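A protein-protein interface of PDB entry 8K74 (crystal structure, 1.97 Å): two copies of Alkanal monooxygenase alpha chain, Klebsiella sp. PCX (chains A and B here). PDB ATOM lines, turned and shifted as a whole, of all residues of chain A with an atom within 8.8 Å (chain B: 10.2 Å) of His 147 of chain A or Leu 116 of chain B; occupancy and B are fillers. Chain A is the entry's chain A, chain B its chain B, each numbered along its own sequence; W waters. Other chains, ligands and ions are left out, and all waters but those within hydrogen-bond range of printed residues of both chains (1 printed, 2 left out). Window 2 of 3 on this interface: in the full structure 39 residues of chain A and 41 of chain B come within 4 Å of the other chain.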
ATOM      1  N   LEU A  85      27.478  35.527   9.560  1.00  0.00           N
ATOM      2  CA  LEU A  85      26.140  35.113   9.976  1.00  0.00           C
ATOM      3  C   LEU A  85      26.190  34.221  11.212  1.00  0.00           C
ATOM      4  O   LEU A  85      25.345  34.340  12.112  1.00  0.00           O
ATOM      5  CB  LEU A  85      25.428  34.408   8.826  1.00  0.00           C
ATOM      6  CG  LEU A  85      23.966  34.067   9.096  1.00  0.00           C
ATOM      7  CD1 LEU A  85      23.171  35.281   9.585  1.00  0.00           C
ATOM      8  CD2 LEU A  85      23.366  33.524   7.815  1.00  0.00           C
ATOM      9  N   GLY A 142      16.921  42.100  11.720  1.00  0.00           N
ATOM     10  CA  GLY A 142      15.822  41.298  11.238  1.00  0.00           C
ATOM     11  C   GLY A 142      15.594  41.335   9.738  1.00  0.00           C
ATOM     12  O   GLY A 142      14.536  40.884   9.288  1.00  0.00           O
ATOM     13  N   ASP A 143      16.539  41.857   8.957  1.00  0.00           N
ATOM     14  CA  ASP A 143      16.401  41.839   7.507  1.00  0.00           C
ATOM     15  C   ASP A 143      16.424  40.409   6.993  1.00  0.00           C
ATOM     16  O   ASP A 143      16.855  39.485   7.692  1.00  0.00           O
ATOM     17  CB  ASP A 143      17.525  42.601   6.810  1.00  0.00           C
ATOM     18  CG  ASP A 143      17.650  44.026   7.277  1.00  0.00           C
ATOM     19  OD1 ASP A 143      16.688  44.574   7.861  1.00  0.00           O
ATOM     20  OD2 ASP A 143      18.707  44.622   6.995  1.00  0.00           O
ATOM     21  N   THR A 144      15.960  40.232   5.751  1.00  0.00           N
ATOM     22  CA  THR A 144      16.007  38.918   5.131  1.00  0.00           C
ATOM     23  C   THR A 144      17.454  38.567   4.804  1.00  0.00           C
ATOM     24  O   THR A 144      18.279  39.438   4.513  1.00  0.00           O
ATOM     25  CB  THR A 144      15.166  38.863   3.851  1.00  0.00           C
ATOM     26  OG1 THR A 144      15.700  39.781   2.904  1.00  0.00           O
ATOM     27  CG2 THR A 144      13.705  39.235   4.127  1.00  0.00           C
ATOM     28  N   LEU A 145      17.751  37.272   4.843  1.00  0.00           N
ATOM     29  CA  LEU A 145      19.114  36.766   4.714  1.00  0.00           C
ATOM     30  C   LEU A 145      19.161  35.935   3.432  1.00  0.00           C
ATOM     31  O   LEU A 145      18.874  34.737   3.454  1.00  0.00           O
ATOM     32  CB  LEU A 145      19.502  35.957   5.980  1.00  0.00           C
ATOM     33  CG  LEU A 145      19.462  36.780   7.285  1.00  0.00           C
ATOM     34  CD1 LEU A 145      19.622  35.936   8.553  1.00  0.00           C
ATOM     35  CD2 LEU A 145      20.499  37.891   7.275  1.00  0.00           C
ATOM     36  N   SER A 146      19.505  36.587   2.316  1.00  0.00           N
ATOM     37  CA  SER A 146      19.626  35.964   0.992  1.00  0.00           C
ATOM     38  C   SER A 146      18.353  35.306   0.459  1.00  0.00           C
ATOM     39  O   SER A 146      18.384  34.694  -0.614  1.00  0.00           O
ATOM     40  CB  SER A 146      20.755  34.924   0.967  1.00  0.00           C
ATOM     41  OG  SER A 146      21.924  35.367   1.633  1.00  0.00           O
ATOM     42  N   HIS A 147      17.238  35.431   1.167  1.00  0.00           N
ATOM     43  CA  HIS A 147      15.972  34.858   0.722  1.00  0.00           C
ATOM     44  C   HIS A 147      14.858  35.353   1.633  1.00  0.00           C
ATOM     45  O   HIS A 147      15.081  35.543   2.835  1.00  0.00           O
ATOM     46  CB  HIS A 147      16.012  33.325   0.739  1.00  0.00           C
ATOM     47  CG  HIS A 147      14.900  32.679  -0.032  1.00  0.00           C
ATOM     48  ND1 HIS A 147      13.666  32.402   0.522  1.00  0.00           N
ATOM     49  CD2 HIS A 147      14.847  32.231  -1.311  1.00  0.00           C
ATOM     50  CE1 HIS A 147      12.895  31.832  -0.388  1.00  0.00           C
ATOM     51  NE2 HIS A 147      13.589  31.713  -1.508  1.00  0.00           N
ATOM     52  N   PRO A 148      13.645  35.550   1.113  1.00  0.00           N
ATOM     53  CA  PRO A 148      12.584  36.131   1.951  1.00  0.00           C
ATOM     54  C   PRO A 148      12.138  35.250   3.116  1.00  0.00           C
ATOM     55  O   PRO A 148      11.587  35.793   4.081  1.00  0.00           O
ATOM     56  CB  PRO A 148      11.438  36.360   0.956  1.00  0.00           C
ATOM     57  CG  PRO A 148      12.136  36.540  -0.375  1.00  0.00           C
ATOM     58  CD  PRO A 148      13.302  35.580  -0.319  1.00  0.00           C
ATOM     59  N   ASP A 149      12.323  33.926   3.079  1.00  0.00           N
ATOM     60  CA  ASP A 149      11.924  33.135   4.246  1.00  0.00           C
ATOM     61  C   ASP A 149      13.009  33.002   5.307  1.00  0.00           C
ATOM     62  O   ASP A 149      12.781  32.300   6.301  1.00  0.00           O
ATOM     63  CB  ASP A 149      11.451  31.728   3.872  1.00  0.00           C
ATOM     64  CG  ASP A 149      10.655  31.684   2.594  1.00  0.00           C
ATOM     65  OD1 ASP A 149       9.519  32.213   2.586  1.00  0.00           O
ATOM     66  OD2 ASP A 149      11.128  31.046   1.636  1.00  0.00           O
ATOM     67  N   ASN A 150      14.159  33.658   5.136  1.00  0.00           N
ATOM     68  CA  ASN A 150      15.267  33.602   6.089  1.00  0.00           C
ATOM     69  C   ASN A 150      15.338  34.901   6.892  1.00  0.00           C
ATOM     70  O   ASN A 150      15.750  35.942   6.364  1.00  0.00           O
ATOM     71  CB  ASN A 150      16.587  33.354   5.368  1.00  0.00           C
ATOM     72  CG  ASN A 150      16.646  31.985   4.718  1.00  0.00           C
ATOM     73  OD1 ASN A 150      15.908  31.065   5.088  1.00  0.00           O
ATOM     74  ND2 ASN A 150      17.472  31.868   3.698  1.00  0.00           N
ATOM     75  N   HIS A 151      14.950  34.830   8.167  1.00  0.00           N
ATOM     76  CA  HIS A 151      15.232  35.869   9.151  1.00  0.00           C
ATOM     77  C   HIS A 151      15.967  35.235  10.326  1.00  0.00           C
ATOM     78  O   HIS A 151      15.684  34.094  10.690  1.00  0.00           O
ATOM     79  CB  HIS A 151      13.958  36.532   9.657  1.00  0.00           C
ATOM     80  CG  HIS A 151      13.132  37.167   8.582  1.00  0.00           C
ATOM     81  ND1 HIS A 151      13.250  38.496   8.235  1.00  0.00           N
ATOM     82  CD2 HIS A 151      12.153  36.658   7.796  1.00  0.00           C
ATOM     83  CE1 HIS A 151      12.386  38.777   7.275  1.00  0.00           C
ATOM     84  NE2 HIS A 151      11.704  37.680   6.994  1.00  0.00           N
ATOM     85  N   LEU A 152      16.892  35.981  10.927  1.00  0.00           N
ATOM     86  CA  LEU A 152      17.666  35.466  12.051  1.00  0.00           C
ATOM     87  C   LEU A 152      16.770  35.002  13.195  1.00  0.00           C
ATOM     88  O   LEU A 152      15.864  35.725  13.618  1.00  0.00           O
ATOM     89  CB  LEU A 152      18.629  36.546  12.547  1.00  0.00           C
ATOM     90  CG  LEU A 152      19.357  36.259  13.861  1.00  0.00           C
ATOM     91  CD1 LEU A 152      20.422  35.222  13.610  1.00  0.00           C
ATOM     92  CD2 LEU A 152      19.993  37.546  14.386  1.00  0.00           C
ATOM     93  N   HIS B  45      18.442  26.681  11.714  1.00  0.00           N
ATOM     94  CA  HIS B  45      18.600  28.090  11.372  1.00  0.00           C
ATOM     95  C   HIS B  45      17.289  28.677  10.856  1.00  0.00           C
ATOM     96  O   HIS B  45      16.593  28.045  10.060  1.00  0.00           O
ATOM     97  CB  HIS B  45      19.667  28.280  10.285  1.00  0.00           C
ATOM     98  CG  HIS B  45      21.022  27.760  10.655  1.00  0.00           C
ATOM     99  ND1 HIS B  45      21.940  28.505  11.364  1.00  0.00           N
ATOM    100  CD2 HIS B  45      21.621  26.574  10.397  1.00  0.00           C
ATOM    101  CE1 HIS B  45      23.041  27.798  11.537  1.00  0.00           C
ATOM    102  NE2 HIS B  45      22.873  26.623  10.958  1.00  0.00           N
ATOM    103  N   PHE B  46      16.968  29.896  11.298  1.00  0.00           N
ATOM    104  CA  PHE B  46      15.970  30.793  10.700  1.00  0.00           C
ATOM    105  C   PHE B  46      14.512  30.392  10.912  1.00  0.00           C
ATOM    106  O   PHE B  46      13.616  31.098  10.424  1.00  0.00           O
ATOM    107  CB  PHE B  46      16.169  30.962   9.185  1.00  0.00           C
ATOM    108  CG  PHE B  46      17.603  31.073   8.773  1.00  0.00           C
ATOM    109  CD1 PHE B  46      18.412  32.056   9.317  1.00  0.00           C
ATOM    110  CD2 PHE B  46      18.133  30.214   7.825  1.00  0.00           C
ATOM    111  CE1 PHE B  46      19.735  32.168   8.947  1.00  0.00           C
ATOM    112  CE2 PHE B  46      19.463  30.316   7.443  1.00  0.00           C
ATOM    113  CZ  PHE B  46      20.262  31.305   7.995  1.00  0.00           C
ATOM    114  N   HIS B  47      14.222  29.314  11.615  1.00  0.00           N
ATOM    115  CA  HIS B  47      12.847  28.809  11.636  1.00  0.00           C
ATOM    116  C   HIS B  47      12.480  28.392  13.056  1.00  0.00           C
ATOM    117  O   HIS B  47      12.874  27.324  13.525  1.00  0.00           O
ATOM    118  CB  HIS B  47      12.677  27.677  10.635  1.00  0.00           C
ATOM    119  CG  HIS B  47      12.867  28.110   9.212  1.00  0.00           C
ATOM    120  ND1 HIS B  47      12.001  28.975   8.576  1.00  0.00           N
ATOM    121  CD2 HIS B  47      13.843  27.831   8.315  1.00  0.00           C
ATOM    122  CE1 HIS B  47      12.424  29.194   7.345  1.00  0.00           C
ATOM    123  NE2 HIS B  47      13.538  28.511   7.158  1.00  0.00           N
ATOM    124  N   PRO B  80      27.603  21.680   6.330  1.00  0.00           N
ATOM    125  CA  PRO B  80      27.746  22.505   5.118  1.00  0.00           C
ATOM    126  C   PRO B  80      27.460  23.972   5.353  1.00  0.00           C
ATOM    127  O   PRO B  80      27.922  24.810   4.574  1.00  0.00           O
ATOM    128  CB  PRO B  80      26.744  21.877   4.143  1.00  0.00           C
ATOM    129  CG  PRO B  80      26.606  20.457   4.615  1.00  0.00           C
ATOM    130  CD  PRO B  80      26.673  20.552   6.107  1.00  0.00           C
ATOM    131  N   MET B  81      26.760  24.305   6.434  1.00  0.00           N
ATOM    132  CA  MET B  81      26.354  25.665   6.788  1.00  0.00           C
ATOM    133  C   MET B  81      27.296  26.259   7.820  1.00  0.00           C
ATOM    134  O   MET B  81      26.846  26.922   8.767  1.00  0.00           O
ATOM    135  CB  MET B  81      24.939  25.599   7.336  1.00  0.00           C
ATOM    136  CG  MET B  81      23.929  25.228   6.269  1.00  0.00           C
ATOM    137  SD  MET B  81      22.236  25.587   6.734  1.00  0.00           S
ATOM    138  CE  MET B  81      21.537  23.951   6.662  1.00  0.00           C
ATOM    139  N   GLY B 110      18.979  19.702   5.348  1.00  0.00           N
ATOM    140  CA  GLY B 110      18.321  20.897   5.831  1.00  0.00           C
ATOM    141  C   GLY B 110      17.409  21.470   4.775  1.00  0.00           C
ATOM    142  O   GLY B 110      17.376  21.021   3.627  1.00  0.00           O
ATOM    143  N   THR B 111      16.658  22.478   5.196  1.00  0.00           N
ATOM    144  CA  THR B 111      15.732  23.143   4.299  1.00  0.00           C
ATOM    145  C   THR B 111      16.523  23.795   3.175  1.00  0.00           C
ATOM    146  O   THR B 111      17.507  24.495   3.449  1.00  0.00           O
ATOM    147  CB  THR B 111      14.929  24.193   5.062  1.00  0.00           C
ATOM    148  OG1 THR B 111      14.111  23.539   6.039  1.00  0.00           O
ATOM    149  CG2 THR B 111      14.055  24.997   4.101  1.00  0.00           C
ATOM    150  N   PRO B 112      16.155  23.572   1.910  1.00  0.00           N
ATOM    151  CA  PRO B 112      16.962  24.125   0.807  1.00  0.00           C
ATOM    152  C   PRO B 112      17.205  25.625   0.907  1.00  0.00           C
ATOM    153  O   PRO B 112      18.339  26.077   0.703  1.00  0.00           O
ATOM    154  CB  PRO B 112      16.157  23.738  -0.444  1.00  0.00           C
ATOM    155  CG  PRO B 112      15.353  22.558  -0.040  1.00  0.00           C
ATOM    156  CD  PRO B 112      15.117  22.637   1.445  1.00  0.00           C
ATOM    157  N   THR B 113      16.191  26.417   1.261  1.00  0.00           N
ATOM    158  CA  THR B 113      16.402  27.860   1.319  1.00  0.00           C
ATOM    159  C   THR B 113      17.345  28.278   2.450  1.00  0.00           C
ATOM    160  O   THR B 113      17.885  29.386   2.403  1.00  0.00           O
ATOM    161  CB  THR B 113      15.048  28.586   1.420  1.00  0.00           C
ATOM    162  OG1 THR B 113      14.541  28.478   2.748  1.00  0.00           O
ATOM    163  CG2 THR B 113      14.042  28.001   0.445  1.00  0.00           C
ATOM    164  N   SER B 114      17.585  27.418   3.445  1.00  0.00           N
ATOM    165  CA  SER B 114      18.507  27.781   4.519  1.00  0.00           C
ATOM    166  C   SER B 114      19.970  27.703   4.107  1.00  0.00           C
ATOM    167  O   SER B 114      20.812  28.303   4.784  1.00  0.00           O
ATOM    168  CB  SER B 114      18.284  26.905   5.757  1.00  0.00           C
ATOM    169  OG  SER B 114      16.921  26.896   6.150  1.00  0.00           O
ATOM    170  N   PHE B 115      20.292  26.994   3.020  1.00  0.00           N
ATOM    171  CA  PHE B 115      21.676  26.934   2.550  1.00  0.00           C
ATOM    172  C   PHE B 115      22.121  28.252   1.928  1.00  0.00           C
ATOM    173  O   PHE B 115      23.303  28.618   2.029  1.00  0.00           O
ATOM    174  CB  PHE B 115      21.842  25.792   1.540  1.00  0.00           C
ATOM    175  CG  PHE B 115      21.760  24.419   2.153  1.00  0.00           C
ATOM    176  CD1 PHE B 115      20.544  23.764   2.260  1.00  0.00           C
ATOM    177  CD2 PHE B 115      22.893  23.795   2.641  1.00  0.00           C
ATOM    178  CE1 PHE B 115      20.463  22.502   2.820  1.00  0.00           C
ATOM    179  CE2 PHE B 115      22.823  22.532   3.212  1.00  0.00           C
ATOM    180  CZ  PHE B 115      21.606  21.887   3.306  1.00  0.00           C
ATOM    181  N   LEU B 116      21.185  28.980   1.301  1.00  0.00           N
ATOM    182  CA  LEU B 116      21.532  30.162   0.509  1.00  0.00           C
ATOM    183  C   LEU B 116      22.313  31.216   1.282  1.00  0.00           C
ATOM    184  O   LEU B 116      23.293  31.743   0.730  1.00  0.00           O
ATOM    185  CB  LEU B 116      20.256  30.762  -0.090  1.00  0.00           C
ATOM    186  CG  LEU B 116      19.464  29.777  -0.957  1.00  0.00           C
ATOM    187  CD1 LEU B 116      18.162  30.406  -1.451  1.00  0.00           C
ATOM    188  CD2 LEU B 116      20.343  29.355  -2.122  1.00  0.00           C
ATOM    189  N   PRO B 117      21.950  31.580   2.518  1.00  0.00           N
ATOM    190  CA  PRO B 117      22.760  32.557   3.267  1.00  0.00           C
ATOM    191  C   PRO B 117      24.196  32.132   3.495  1.00  0.00           C
ATOM    192  O   PRO B 117      25.022  32.982   3.857  1.00  0.00           O
ATOM    193  CB  PRO B 117      22.023  32.664   4.608  1.00  0.00           C
ATOM    194  CG  PRO B 117      20.658  32.244   4.325  1.00  0.00           C
ATOM    195  CD  PRO B 117      20.777  31.160   3.300  1.00  0.00           C
ATOM    196  N   PHE B 118      24.519  30.848   3.346  1.00  0.00           N
ATOM    197  CA  PHE B 118      25.860  30.352   3.637  1.00  0.00           C
ATOM    198  C   PHE B 118      26.659  30.047   2.375  1.00  0.00           C
ATOM    199  O   PHE B 118      27.666  29.341   2.440  1.00  0.00           O
ATOM    200  CB  PHE B 118      25.796  29.123   4.546  1.00  0.00           C
ATOM    201  CG  PHE B 118      25.119  29.387   5.854  1.00  0.00           C
ATOM    202  CD1 PHE B 118      25.790  30.059   6.863  1.00  0.00           C
ATOM    203  CD2 PHE B 118      23.807  28.987   6.073  1.00  0.00           C
ATOM    204  CE1 PHE B 118      25.158  30.331   8.075  1.00  0.00           C
ATOM    205  CE2 PHE B 118      23.178  29.239   7.280  1.00  0.00           C
ATOM    206  CZ  PHE B 118      23.849  29.913   8.283  1.00  0.00           C
ATOM    207  N   GLY B 119      26.245  30.586   1.234  1.00  0.00           N
ATOM    208  CA  GLY B 119      27.075  30.507   0.051  1.00  0.00           C
ATOM    209  C   GLY B 119      27.064  29.180  -0.672  1.00  0.00           C
ATOM    210  O   GLY B 119      28.027  28.865  -1.380  1.00  0.00           O
ATOM    211  N   LEU B 120      26.010  28.382  -0.516  1.00  0.00           N
ATOM    212  CA  LEU B 120      25.880  27.146  -1.272  1.00  0.00           C
ATOM    213  C   LEU B 120      24.408  26.832  -1.460  1.00  0.00           C
ATOM    214  O   LEU B 120      23.529  27.461  -0.864  1.00  0.00           O
ATOM    215  CB  LEU B 120      26.586  25.953  -0.608  1.00  0.00           C
ATOM    216  CG  LEU B 120      25.919  25.250   0.590  1.00  0.00           C
ATOM    217  CD1 LEU B 120      26.808  24.165   1.176  1.00  0.00           C
ATOM    218  CD2 LEU B 120      25.653  26.264   1.689  1.00  0.00           C
ATOM    219  N   THR B 121      24.147  25.826  -2.282  1.00  0.00           N
ATOM    220  CA  THR B 121      22.800  25.314  -2.470  1.00  0.00           C
ATOM    221  C   THR B 121      22.708  23.914  -1.889  1.00  0.00           C
ATOM    222  O   THR B 121      23.719  23.279  -1.572  1.00  0.00           O
ATOM    223  CB  THR B 121      22.418  25.292  -3.952  1.00  0.00           C
ATOM    224  OG1 THR B 121      23.082  24.195  -4.593  1.00  0.00           O
ATOM    225  CG2 THR B 121      22.805  26.603  -4.617  1.00  0.00           C
ATOM    226  N   SER B 122      21.470  23.439  -1.769  1.00  0.00           N
ATOM    227  CA  SER B 122      21.220  22.137  -1.165  1.00  0.00           C
ATOM    228  C   SER B 122      21.794  21.001  -2.004  1.00  0.00           C
ATOM    229  O   SER B 122      22.207  19.973  -1.451  1.00  0.00           O
ATOM    230  CB  SER B 122      19.713  21.953  -0.949  1.00  0.00           C
ATOM    231  OG  SER B 122      19.339  20.589  -0.963  1.00  0.00           O
ATOM    232  N   GLU B 123      21.837  21.166  -3.339  1.00  0.00           N
ATOM    233  CA  GLU B 123      22.439  20.149  -4.200  1.00  0.00           C
ATOM    234  C   GLU B 123      23.937  20.011  -3.966  1.00  0.00           C
ATOM    235  O   GLU B 123      24.524  19.009  -4.383  1.00  0.00           O
ATOM    236  CB  GLU B 123      22.188  20.464  -5.686  1.00  0.00           C
ATOM    237  N   GLN B 124      24.575  20.989  -3.326  1.00  0.00           N
ATOM    238  CA  GLN B 124      26.009  20.914  -3.065  1.00  0.00           C
ATOM    239  C   GLN B 124      26.336  20.369  -1.680  1.00  0.00           C
ATOM    240  O   GLN B 124      27.520  20.253  -1.340  1.00  0.00           O
ATOM    241  CB  GLN B 124      26.656  22.291  -3.223  1.00  0.00           C
ATOM    242  CG  GLN B 124      26.517  22.884  -4.618  1.00  0.00           C
ATOM    243  CD  GLN B 124      27.016  24.301  -4.673  1.00  0.00           C
ATOM    244  OE1 GLN B 124      26.540  25.177  -3.942  1.00  0.00           O
ATOM    245  NE2 GLN B 124      27.989  24.544  -5.552  1.00  0.00           N
ATOM    246  N   ARG B 125      25.323  20.007  -0.894  1.00  0.00           N
ATOM    247  CA  ARG B 125      25.542  19.731   0.526  1.00  0.00           C
ATOM    248  C   ARG B 125      26.459  18.532   0.746  1.00  0.00           C
ATOM    249  O   ARG B 125      27.308  18.561   1.640  1.00  0.00           O
ATOM    250  CB  ARG B 125      24.199  19.543   1.237  1.00  0.00           C
ATOM    251  CG  ARG B 125      23.472  18.191   1.023  1.00  0.00           C
ATOM    252  CD  ARG B 125      21.989  18.311   1.480  1.00  0.00           C
ATOM    253  NE  ARG B 125      21.229  17.085   1.239  1.00  0.00           N
ATOM    254  CZ  ARG B 125      20.611  16.810   0.099  1.00  0.00           C
ATOM    255  NH1 ARG B 125      20.682  17.627  -0.940  1.00  0.00           N
ATOM    256  NH2 ARG B 125      19.913  15.679  -0.005  1.00  0.00           N
HETATM  257  O   HOH W   1      13.177  33.595  11.978  1.00  0.00           O
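Of the 12 printed residues of chain A, 7 touch a printed residue of chain B. Hydrophobic or aromatic side chains of chain A within 4 Å of the printed part of chain B: Leu 85, Leu 145 and His 147. Along chain A the printed residues that touch a printed residue of chain B span positions 85 to 151. Of the 21 printed residues of chain B, 6 touch a printed residue of chain A. Printed residues of chain B that touch a printed residue of chain A: Phe 46, His 47, Thr 113, Leu 116, Pro 117 and Phe 118. Hydrophobic or aromatic side chains of chain B that line the printed part of chain A: Phe 46, His 47, Leu 116, Pro 117 and Phe 118.
The side-chain amide nitrogen of Asn 150 of chain A is in hydrogen-bond range of the backbone carbonyl oxygen of Thr 113 of chain B (2.8 Å).
Of the printed residues of chain B, Leu 85 of chain A touches Phe 46, Pro 117 and Phe 118. His 147 of chain A touches just one residue of chain B: Leu 116. No residue of chain B comes within 4 Å of Pro 148 of chain A. Asp 149 of chain A touches just one residue of chain B: His 47. Asn 150 of chain A touches just these residues of chain B: Phe 46 (3.6 Å), Thr 113 (2.8 Å) and Pro 117 (3.3 Å). Of the printed residues of chain B, His 151 of chain A touches Phe 46. Printed residues of chain A within 4 Å of Phe 46 of chain B: Leu 85, Leu 145, Asn 150 and His 151. Of the printed residues of chain A, Thr 113 of chain B touches Asn 150 (2.8 Å). Of the printed residues of chain A, Leu 116 of chain B touches Ser 146 (3.98 Å) and His 147 (3.8 Å). Of chain A, only Leu 85 (3.6 Å), Leu 145 (3.2 Å), Ser 146 (3.4 Å) and Asn 150 (3.3 Å) come within 4 Å of Pro 117 of chain B. The nearest residue of chain A that does not touch Leu 116 of chain B is Asn 150 of chain A (4.8 Å).
A ring nitrogen (ND1) of His 151 of chain A is in hydrogen-bond range of the backbone carbonyl oxygen (O) of Gly 142 of chain A, 2.9 Å away. The backbone carbonyl oxygen (O) of Asn 150 of chain A sits at hydrogen-bond distance from the backbone NH (N) of Leu 145 of chain A, at 2.8 Å. A ring nitrogen (ND1) of His 147 of chain A lies close to the side-chain carboxylate (OD2) of Asp 149 of chain A (3.1 Å). The backbone carbonyl oxygen (O) of Pro 148 of chain A is in hydrogen-bond range of a ring nitrogen (NE2) of His 151 of chain A, 3.5 Å away.
Water W1 lies within hydrogen-bond range of the backbone carbonyl oxygen of His 151 of chain A and the backbone carbonyl oxygen of Phe 46 of chain B.
CB of Pro 117 of chain B touches CD2 of Leu 85 of chain A (3.6 Å). Leu 85 of chain A touches Phe 118 of chain B (CD2 to CE1, 3.7 Å). CE1 of Phe 46 of chain B touches CD1 of Leu 145 of chain A, at 3.8 Å. CG of Pro 117 of chain B touches O of Leu 145 of chain A, at 3.2 Å. Ser 146 of chain A touches Leu 116 of chain B (OG to O, 3.98 Å). Ser 146 of chain A touches Pro 117 of chain B (OG to CA, 3.4 Å). Leu 116 of chain B touches His 147 of chain A. Phe 46 of chain B touches Asn 150 of chain A. ND2 of Asn 150 of chain A touches CG of Pro 117 of chain B (3.3 Å). Phe 46 of chain B touches His 151 of chain A.
No position is printed for both chains.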
